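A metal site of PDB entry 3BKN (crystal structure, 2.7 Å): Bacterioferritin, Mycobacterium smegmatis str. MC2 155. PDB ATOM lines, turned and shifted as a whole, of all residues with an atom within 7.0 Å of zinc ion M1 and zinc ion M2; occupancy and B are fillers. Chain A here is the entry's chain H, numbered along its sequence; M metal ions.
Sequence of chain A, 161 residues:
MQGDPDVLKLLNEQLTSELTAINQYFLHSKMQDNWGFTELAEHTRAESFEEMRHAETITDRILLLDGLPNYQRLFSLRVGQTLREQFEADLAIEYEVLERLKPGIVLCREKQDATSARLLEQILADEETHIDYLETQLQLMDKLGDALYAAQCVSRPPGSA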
ATOM      1  N   GLN A  14     -11.850   2.416 -25.956  1.00  0.00           N
ATOM      2  CA  GLN A  14     -12.225   1.027 -26.151  1.00  0.00           C
ATOM      3  C   GLN A  14     -12.475   0.745 -27.627  1.00  0.00           C
ATOM      4  O   GLN A  14     -12.042  -0.278 -28.142  1.00  0.00           O
ATOM      5  CB  GLN A  14     -13.462   0.693 -25.330  1.00  0.00           C
ATOM      6  CG  GLN A  14     -13.754  -0.788 -25.282  1.00  0.00           C
ATOM      7  CD  GLN A  14     -12.535  -1.571 -24.954  1.00  0.00           C
ATOM      8  OE1 GLN A  14     -11.678  -1.069 -24.220  1.00  0.00           O
ATOM      9  NE2 GLN A  14     -12.420  -2.799 -25.486  1.00  0.00           N
ATOM     10  N   SER A  17      -9.412   0.300 -29.512  1.00  0.00           N
ATOM     11  CA  SER A  17      -8.808  -0.996 -29.226  1.00  0.00           C
ATOM     12  C   SER A  17      -9.513  -2.120 -30.003  1.00  0.00           C
ATOM     13  O   SER A  17      -8.857  -2.998 -30.549  1.00  0.00           O
ATOM     14  CB  SER A  17      -8.658  -1.164 -27.712  1.00  0.00           C
ATOM     15  OG  SER A  17      -8.626  -2.515 -27.358  1.00  0.00           O
ATOM     16  N   GLU A  18     -10.840  -2.021 -30.140  1.00  0.00           N
ATOM     17  CA  GLU A  18     -11.565  -2.989 -30.969  1.00  0.00           C
ATOM     18  C   GLU A  18     -11.166  -2.858 -32.442  1.00  0.00           C
ATOM     19  O   GLU A  18     -10.979  -3.884 -33.138  1.00  0.00           O
ATOM     20  CB  GLU A  18     -13.100  -2.878 -30.824  1.00  0.00           C
ATOM     21  CG  GLU A  18     -13.686  -2.823 -29.411  1.00  0.00           C
ATOM     22  CD  GLU A  18     -13.610  -4.142 -28.633  1.00  0.00           C
ATOM     23  OE1 GLU A  18     -13.330  -5.189 -29.232  1.00  0.00           O
ATOM     24  OE2 GLU A  18     -13.830  -4.126 -27.408  1.00  0.00           O
ATOM     25  N   ALA A  21      -7.975  -4.544 -32.819  1.00  0.00           N
ATOM     26  CA  ALA A  21      -8.062  -6.015 -32.728  1.00  0.00           C
ATOM     27  C   ALA A  21      -8.708  -6.663 -33.972  1.00  0.00           C
ATOM     28  O   ALA A  21      -8.270  -7.703 -34.397  1.00  0.00           O
ATOM     29  CB  ALA A  21      -8.732  -6.480 -31.422  1.00  0.00           C
ATOM     30  N   TYR A  25      -6.441  -9.535 -35.715  1.00  0.00           N
ATOM     31  CA  TYR A  25      -6.964 -10.878 -35.757  1.00  0.00           C
ATOM     32  C   TYR A  25      -7.213 -11.246 -37.196  1.00  0.00           C
ATOM     33  O   TYR A  25      -6.884 -12.335 -37.636  1.00  0.00           O
ATOM     34  CB  TYR A  25      -8.251 -10.939 -34.964  1.00  0.00           C
ATOM     35  CG  TYR A  25      -8.112 -11.249 -33.507  1.00  0.00           C
ATOM     36  CD1 TYR A  25      -7.819 -12.548 -33.075  1.00  0.00           C
ATOM     37  CD2 TYR A  25      -8.348 -10.297 -32.548  1.00  0.00           C
ATOM     38  CE1 TYR A  25      -7.710 -12.872 -31.728  1.00  0.00           C
ATOM     39  CE2 TYR A  25      -8.242 -10.585 -31.212  1.00  0.00           C
ATOM     40  CZ  TYR A  25      -7.936 -11.888 -30.800  1.00  0.00           C
ATOM     41  OH  TYR A  25      -7.858 -12.230 -29.456  1.00  0.00           O
ATOM     42  N   GLU A  47     -12.660 -14.907 -34.153  1.00  0.00           N
ATOM     43  CA  GLU A  47     -12.304 -13.908 -33.157  1.00  0.00           C
ATOM     44  C   GLU A  47     -12.375 -12.473 -33.769  1.00  0.00           C
ATOM     45  O   GLU A  47     -12.887 -11.536 -33.158  1.00  0.00           O
ATOM     46  CB  GLU A  47     -10.955 -14.245 -32.493  1.00  0.00           C
ATOM     47  CG  GLU A  47     -10.987 -15.402 -31.462  1.00  0.00           C
ATOM     48  CD  GLU A  47      -9.558 -15.771 -30.993  1.00  0.00           C
ATOM     49  OE1 GLU A  47      -9.122 -15.374 -29.861  1.00  0.00           O
ATOM     50  OE2 GLU A  47      -8.840 -16.432 -31.802  1.00  0.00           O
ATOM     51  N   GLU A  50     -15.904 -11.248 -33.849  1.00  0.00           N
ATOM     52  CA  GLU A  50     -16.371 -10.910 -32.539  1.00  0.00           C
ATOM     53  C   GLU A  50     -15.903  -9.484 -32.259  1.00  0.00           C
ATOM     54  O   GLU A  50     -16.677  -8.671 -31.690  1.00  0.00           O
ATOM     55  CB  GLU A  50     -15.902 -11.918 -31.491  1.00  0.00           C
ATOM     56  CG  GLU A  50     -16.697 -11.857 -30.177  1.00  0.00           C
ATOM     57  CD  GLU A  50     -16.577 -13.117 -29.311  1.00  0.00           C
ATOM     58  OE1 GLU A  50     -16.706 -14.254 -29.855  1.00  0.00           O
ATOM     59  OE2 GLU A  50     -16.364 -12.966 -28.087  1.00  0.00           O
ATOM     60  N   GLU A  51     -14.691  -9.139 -32.696  1.00  0.00           N
ATOM     61  CA  GLU A  51     -14.204  -7.807 -32.494  1.00  0.00           C
ATOM     62  C   GLU A  51     -14.992  -6.784 -33.335  1.00  0.00           C
ATOM     63  O   GLU A  51     -15.278  -5.669 -32.885  1.00  0.00           O
ATOM     64  CB  GLU A  51     -12.725  -7.756 -32.763  1.00  0.00           C
ATOM     65  CG  GLU A  51     -11.933  -8.688 -31.847  1.00  0.00           C
ATOM     66  CD  GLU A  51     -12.032  -8.403 -30.332  1.00  0.00           C
ATOM     67  OE1 GLU A  51     -12.383  -7.274 -29.891  1.00  0.00           O
ATOM     68  OE2 GLU A  51     -11.723  -9.335 -29.564  1.00  0.00           O
ATOM     69  N   MET A  52     -15.349  -7.190 -34.546  1.00  0.00           N
ATOM     70  CA  MET A  52     -16.230  -6.373 -35.360  1.00  0.00           C
ATOM     71  C   MET A  52     -17.550  -6.079 -34.618  1.00  0.00           C
ATOM     72  O   MET A  52     -18.018  -4.915 -34.550  1.00  0.00           O
ATOM     73  CB  MET A  52     -16.465  -7.022 -36.693  1.00  0.00           C
ATOM     74  CG  MET A  52     -15.308  -6.878 -37.645  1.00  0.00           C
ATOM     75  SD  MET A  52     -15.511  -7.879 -39.169  1.00  0.00           S
ATOM     76  CE  MET A  52     -13.823  -8.417 -39.376  1.00  0.00           C
ATOM     77  N   ARG A  53     -18.142  -7.114 -34.019  1.00  0.00           N
ATOM     78  CA  ARG A  53     -19.364  -6.873 -33.250  1.00  0.00           C
ATOM     79  C   ARG A  53     -19.193  -5.949 -32.052  1.00  0.00           C
ATOM     80  O   ARG A  53     -20.083  -5.146 -31.785  1.00  0.00           O
ATOM     81  CB  ARG A  53     -20.101  -8.179 -32.927  1.00  0.00           C
ATOM     82  CG  ARG A  53     -20.809  -8.685 -34.198  1.00  0.00           C
ATOM     83  CD  ARG A  53     -21.541 -10.041 -34.050  1.00  0.00           C
ATOM     84  NE  ARG A  53     -20.761 -11.168 -34.577  1.00  0.00           N
ATOM     85  CZ  ARG A  53     -20.126 -12.071 -33.837  1.00  0.00           C
ATOM     86  NH1 ARG A  53     -20.140 -12.004 -32.502  1.00  0.00           N
ATOM     87  NH2 ARG A  53     -19.447 -13.038 -34.439  1.00  0.00           N
ATOM     88  N   HIS A  54     -18.059  -6.044 -31.353  1.00  0.00           N
ATOM     89  CA  HIS A  54     -17.768  -5.130 -30.236  1.00  0.00           C
ATOM     90  C   HIS A  54     -17.645  -3.688 -30.740  1.00  0.00           C
ATOM     91  O   HIS A  54     -18.185  -2.769 -30.125  1.00  0.00           O
ATOM     92  CB  HIS A  54     -16.493  -5.556 -29.537  1.00  0.00           C
ATOM     93  CG  HIS A  54     -16.643  -6.833 -28.769  1.00  0.00           C
ATOM     94  ND1 HIS A  54     -15.580  -7.536 -28.249  1.00  0.00           N
ATOM     95  CD2 HIS A  54     -17.761  -7.532 -28.432  1.00  0.00           C
ATOM     96  CE1 HIS A  54     -16.025  -8.610 -27.607  1.00  0.00           C
ATOM     97  NE2 HIS A  54     -17.339  -8.633 -27.712  1.00  0.00           N
ATOM     98  N   ALA A  55     -16.951  -3.505 -31.865  1.00  0.00           N
ATOM     99  CA  ALA A  55     -16.791  -2.193 -32.410  1.00  0.00           C
ATOM    100  C   ALA A  55     -18.179  -1.618 -32.713  1.00  0.00           C
ATOM    101  O   ALA A  55     -18.446  -0.452 -32.415  1.00  0.00           O
ATOM    102  CB  ALA A  55     -15.876  -2.241 -33.655  1.00  0.00           C
ATOM    103  N   ILE A  58     -20.152  -0.703 -29.406  1.00  0.00           N
ATOM    104  CA  ILE A  58     -19.610   0.544 -28.863  1.00  0.00           C
ATOM    105  C   ILE A  58     -20.011   1.780 -29.680  1.00  0.00           C
ATOM    106  O   ILE A  58     -20.429   2.781 -29.104  1.00  0.00           O
ATOM    107  CB  ILE A  58     -18.066   0.498 -28.622  1.00  0.00           C
ATOM    108  CG1 ILE A  58     -17.778  -0.305 -27.362  1.00  0.00           C
ATOM    109  CG2 ILE A  58     -17.479   1.938 -28.459  1.00  0.00           C
ATOM    110  CD1 ILE A  58     -16.584  -1.117 -27.481  1.00  0.00           C
ATOM    111  N   ASP A  90      -1.851 -11.290 -29.859  1.00  0.00           N
ATOM    112  CA  ASP A  90      -3.273 -11.141 -29.596  1.00  0.00           C
ATOM    113  C   ASP A  90      -3.572 -11.103 -28.106  1.00  0.00           C
ATOM    114  O   ASP A  90      -4.414 -10.358 -27.657  1.00  0.00           O
ATOM    115  CB  ASP A  90      -4.051 -12.241 -30.308  1.00  0.00           C
ATOM    116  CG  ASP A  90      -3.976 -12.106 -31.883  1.00  0.00           C
ATOM    117  OD1 ASP A  90      -3.680 -10.978 -32.384  1.00  0.00           O
ATOM    118  OD2 ASP A  90      -4.226 -13.124 -32.603  1.00  0.00           O
ATOM    119  N   GLU A  94      -5.506  -8.167 -25.622  1.00  0.00           N
ATOM    120  CA  GLU A  94      -6.607  -8.507 -24.753  1.00  0.00           C
ATOM    121  C   GLU A  94      -6.333  -8.049 -23.332  1.00  0.00           C
ATOM    122  O   GLU A  94      -7.249  -7.587 -22.645  1.00  0.00           O
ATOM    123  CB  GLU A  94      -6.920  -9.994 -24.784  1.00  0.00           C
ATOM    124  CG  GLU A  94      -7.305 -10.590 -26.135  1.00  0.00           C
ATOM    125  CD  GLU A  94      -8.575 -10.008 -26.785  1.00  0.00           C
ATOM    126  OE1 GLU A  94      -9.399  -9.319 -26.136  1.00  0.00           O
ATOM    127  OE2 GLU A  94      -8.742 -10.268 -27.985  1.00  0.00           O
ATOM    128  N   VAL A  97      -6.983  -4.444 -22.957  1.00  0.00           N
ATOM    129  CA  VAL A  97      -8.416  -4.244 -22.770  1.00  0.00           C
ATOM    130  C   VAL A  97      -8.812  -4.360 -21.288  1.00  0.00           C
ATOM    131  O   VAL A  97      -9.455  -3.451 -20.740  1.00  0.00           O
ATOM    132  CB  VAL A  97      -9.225  -5.198 -23.667  1.00  0.00           C
ATOM    133  CG1 VAL A  97     -10.689  -5.188 -23.258  1.00  0.00           C
ATOM    134  CG2 VAL A  97      -9.065  -4.784 -25.138  1.00  0.00           C
ATOM    135  N   ILE A 123     -18.429  -6.781 -22.823  1.00  0.00           N
ATOM    136  CA  ILE A 123     -17.212  -6.879 -23.593  1.00  0.00           C
ATOM    137  C   ILE A 123     -16.076  -7.522 -22.749  1.00  0.00           C
ATOM    138  O   ILE A 123     -15.362  -8.404 -23.212  1.00  0.00           O
ATOM    139  CB  ILE A 123     -16.842  -5.539 -24.167  1.00  0.00           C
ATOM    140  CG1 ILE A 123     -17.678  -5.313 -25.425  1.00  0.00           C
ATOM    141  CG2 ILE A 123     -15.347  -5.469 -24.516  1.00  0.00           C
ATOM    142  CD1 ILE A 123     -17.886  -3.836 -25.751  1.00  0.00           C
ATOM    143  N   ASP A 126     -16.408 -11.221 -22.667  1.00  0.00           N
ATOM    144  CA  ASP A 126     -15.946 -11.733 -23.945  1.00  0.00           C
ATOM    145  C   ASP A 126     -14.427 -11.719 -24.028  1.00  0.00           C
ATOM    146  O   ASP A 126     -13.831 -12.705 -24.407  1.00  0.00           O
ATOM    147  CB  ASP A 126     -16.563 -10.953 -25.107  1.00  0.00           C
ATOM    148  CG  ASP A 126     -18.057 -11.286 -25.363  1.00  0.00           C
ATOM    149  OD1 ASP A 126     -18.630 -12.192 -24.698  1.00  0.00           O
ATOM    150  OD2 ASP A 126     -18.682 -10.632 -26.261  1.00  0.00           O
ATOM    151  N   GLU A 127     -13.752 -10.634 -23.637  1.00  0.00           N
ATOM    152  CA  GLU A 127     -12.285 -10.640 -23.758  1.00  0.00           C
ATOM    153  C   GLU A 127     -11.593 -11.602 -22.795  1.00  0.00           C
ATOM    154  O   GLU A 127     -10.552 -12.153 -23.135  1.00  0.00           O
ATOM    155  CB  GLU A 127     -11.653  -9.256 -23.688  1.00  0.00           C
ATOM    156  CG  GLU A 127     -12.406  -8.161 -24.423  1.00  0.00           C
ATOM    157  CD  GLU A 127     -12.334  -8.171 -25.956  1.00  0.00           C
ATOM    158  OE1 GLU A 127     -12.417  -9.204 -26.634  1.00  0.00           O
ATOM    159  OE2 GLU A 127     -12.276  -7.071 -26.503  1.00  0.00           O
ATOM    160  N   GLU A 128     -12.173 -11.808 -21.607  1.00  0.00           N
ATOM    161  CA  GLU A 128     -11.601 -12.715 -20.611  1.00  0.00           C
ATOM    162  C   GLU A 128     -11.599 -14.096 -21.234  1.00  0.00           C
ATOM    163  O   GLU A 128     -10.625 -14.802 -21.137  1.00  0.00           O
ATOM    164  CB  GLU A 128     -12.380 -12.696 -19.282  1.00  0.00           C
ATOM    165  CG  GLU A 128     -12.353 -11.329 -18.584  1.00  0.00           C
ATOM    166  CD  GLU A 128     -12.652 -11.362 -17.056  1.00  0.00           C
ATOM    167  OE1 GLU A 128     -12.576 -12.446 -16.472  1.00  0.00           O
ATOM    168  OE2 GLU A 128     -12.914 -10.308 -16.410  1.00  0.00           O
ATOM    169  N   HIS A 130     -11.457 -14.782 -24.575  1.00  0.00           N
ATOM    170  CA  HIS A 130     -10.348 -14.773 -25.530  1.00  0.00           C
ATOM    171  C   HIS A 130      -9.010 -15.021 -24.816  1.00  0.00           C
ATOM    172  O   HIS A 130      -8.254 -15.922 -25.199  1.00  0.00           O
ATOM    173  CB  HIS A 130     -10.379 -13.536 -26.435  1.00  0.00           C
ATOM    174  CG  HIS A 130     -11.596 -13.480 -27.328  1.00  0.00           C
ATOM    175  ND1 HIS A 130     -12.194 -12.293 -27.717  1.00  0.00           N
ATOM    176  CD2 HIS A 130     -12.343 -14.475 -27.889  1.00  0.00           C
ATOM    177  CE1 HIS A 130     -13.240 -12.562 -28.489  1.00  0.00           C
ATOM    178  NE2 HIS A 130     -13.345 -13.870 -28.613  1.00  0.00           N
ATOM    179  N   ILE A 131      -8.763 -14.290 -23.725  1.00  0.00           N
ATOM    180  CA  ILE A 131      -7.567 -14.488 -22.931  1.00  0.00           C
ATOM    181  C   ILE A 131      -7.400 -15.946 -22.501  1.00  0.00           C
ATOM    182  O   ILE A 131      -6.313 -16.522 -22.614  1.00  0.00           O
ATOM    183  CB  ILE A 131      -7.548 -13.562 -21.726  1.00  0.00           C
ATOM    184  CG1 ILE A 131      -7.487 -12.143 -22.228  1.00  0.00           C
ATOM    185  CG2 ILE A 131      -6.388 -13.913 -20.779  1.00  0.00           C
ATOM    186  CD1 ILE A 131      -7.755 -11.106 -21.174  1.00  0.00           C
ATOM    187  N   LEU A 134      -6.359 -18.072 -25.468  1.00  0.00           N
ATOM    188  CA  LEU A 134      -5.007 -17.759 -25.915  1.00  0.00           C
ATOM    189  C   LEU A 134      -3.997 -18.322 -24.955  1.00  0.00           C
ATOM    190  O   LEU A 134      -3.009 -18.957 -25.365  1.00  0.00           O
ATOM    191  CB  LEU A 134      -4.839 -16.248 -26.055  1.00  0.00           C
ATOM    192  CG  LEU A 134      -5.670 -15.612 -27.169  1.00  0.00           C
ATOM    193  CD1 LEU A 134      -5.746 -14.094 -27.006  1.00  0.00           C
ATOM    194  CD2 LEU A 134      -5.232 -15.999 -28.612  1.00  0.00           C
HETATM  195 ZN    ZN M   1     -11.281 -10.136 -27.872  1.00  0.00          ZN
HETATM  196 ZN    ZN M   2     -13.506  -6.871 -28.203  1.00  0.00          ZN
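OE2 of Glu 18 sits at hydrogen-bond distance from NE2 of Gln 14 (2.7 Å).
NE2 of His 54 is in hydrogen-bond range of OD2 of Asp 126 (2.8 Å).
The side-chain carboxylate (OE2) of Glu 50 sits close to a ring nitrogen (NE2) of His 130 (3.2 Å).
The side-chain carboxylate (OE2) of Glu 94 lies close to the side-chain hydroxyl (OH) of Tyr 25 (2.6 Å).
Within 4 Å of zinc ion M1: Glu 51, Glu 94, Glu 127 and His 130.
Along chain A the residues within 4 Å of zinc ion M1 span positions 51 to 130.
The nearest printed residue that does not touch zinc ion M1 is Tyr 25 (4.3 Å).
Of the 23 residues printed, 4 come within 4 Å of zinc ion M2.
Along chain A the residues within 4 Å of zinc ion M2 span positions 18 to 127.
The nearest printed residue that does not touch zinc ion M2 is Ile 123 (4.4 Å).
OE1 of Glu 127 is bound to zinc ion M1.
OE2 of Glu 51 is bound to zinc ion M1, 1.9 Å away.
ND1 of His 130 is bound to zinc ion M1.
OE2 of Glu 94 binds zinc ion M1, 2.5 Å away.
Zinc ion M1 has four donor atoms within binding distance.
Slightly farther from zinc ion M1 lies the side-chain carboxylate (OE1) of Glu 94 (2.7 Å).
Zinc ion M2 is bound by OE1 of Glu 18 (2.0 Å), OE1 of Glu 51 (2.1 Å), OE2 of Glu 127 (2.1 Å) and ND1 of His 54 (2.2 Å).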
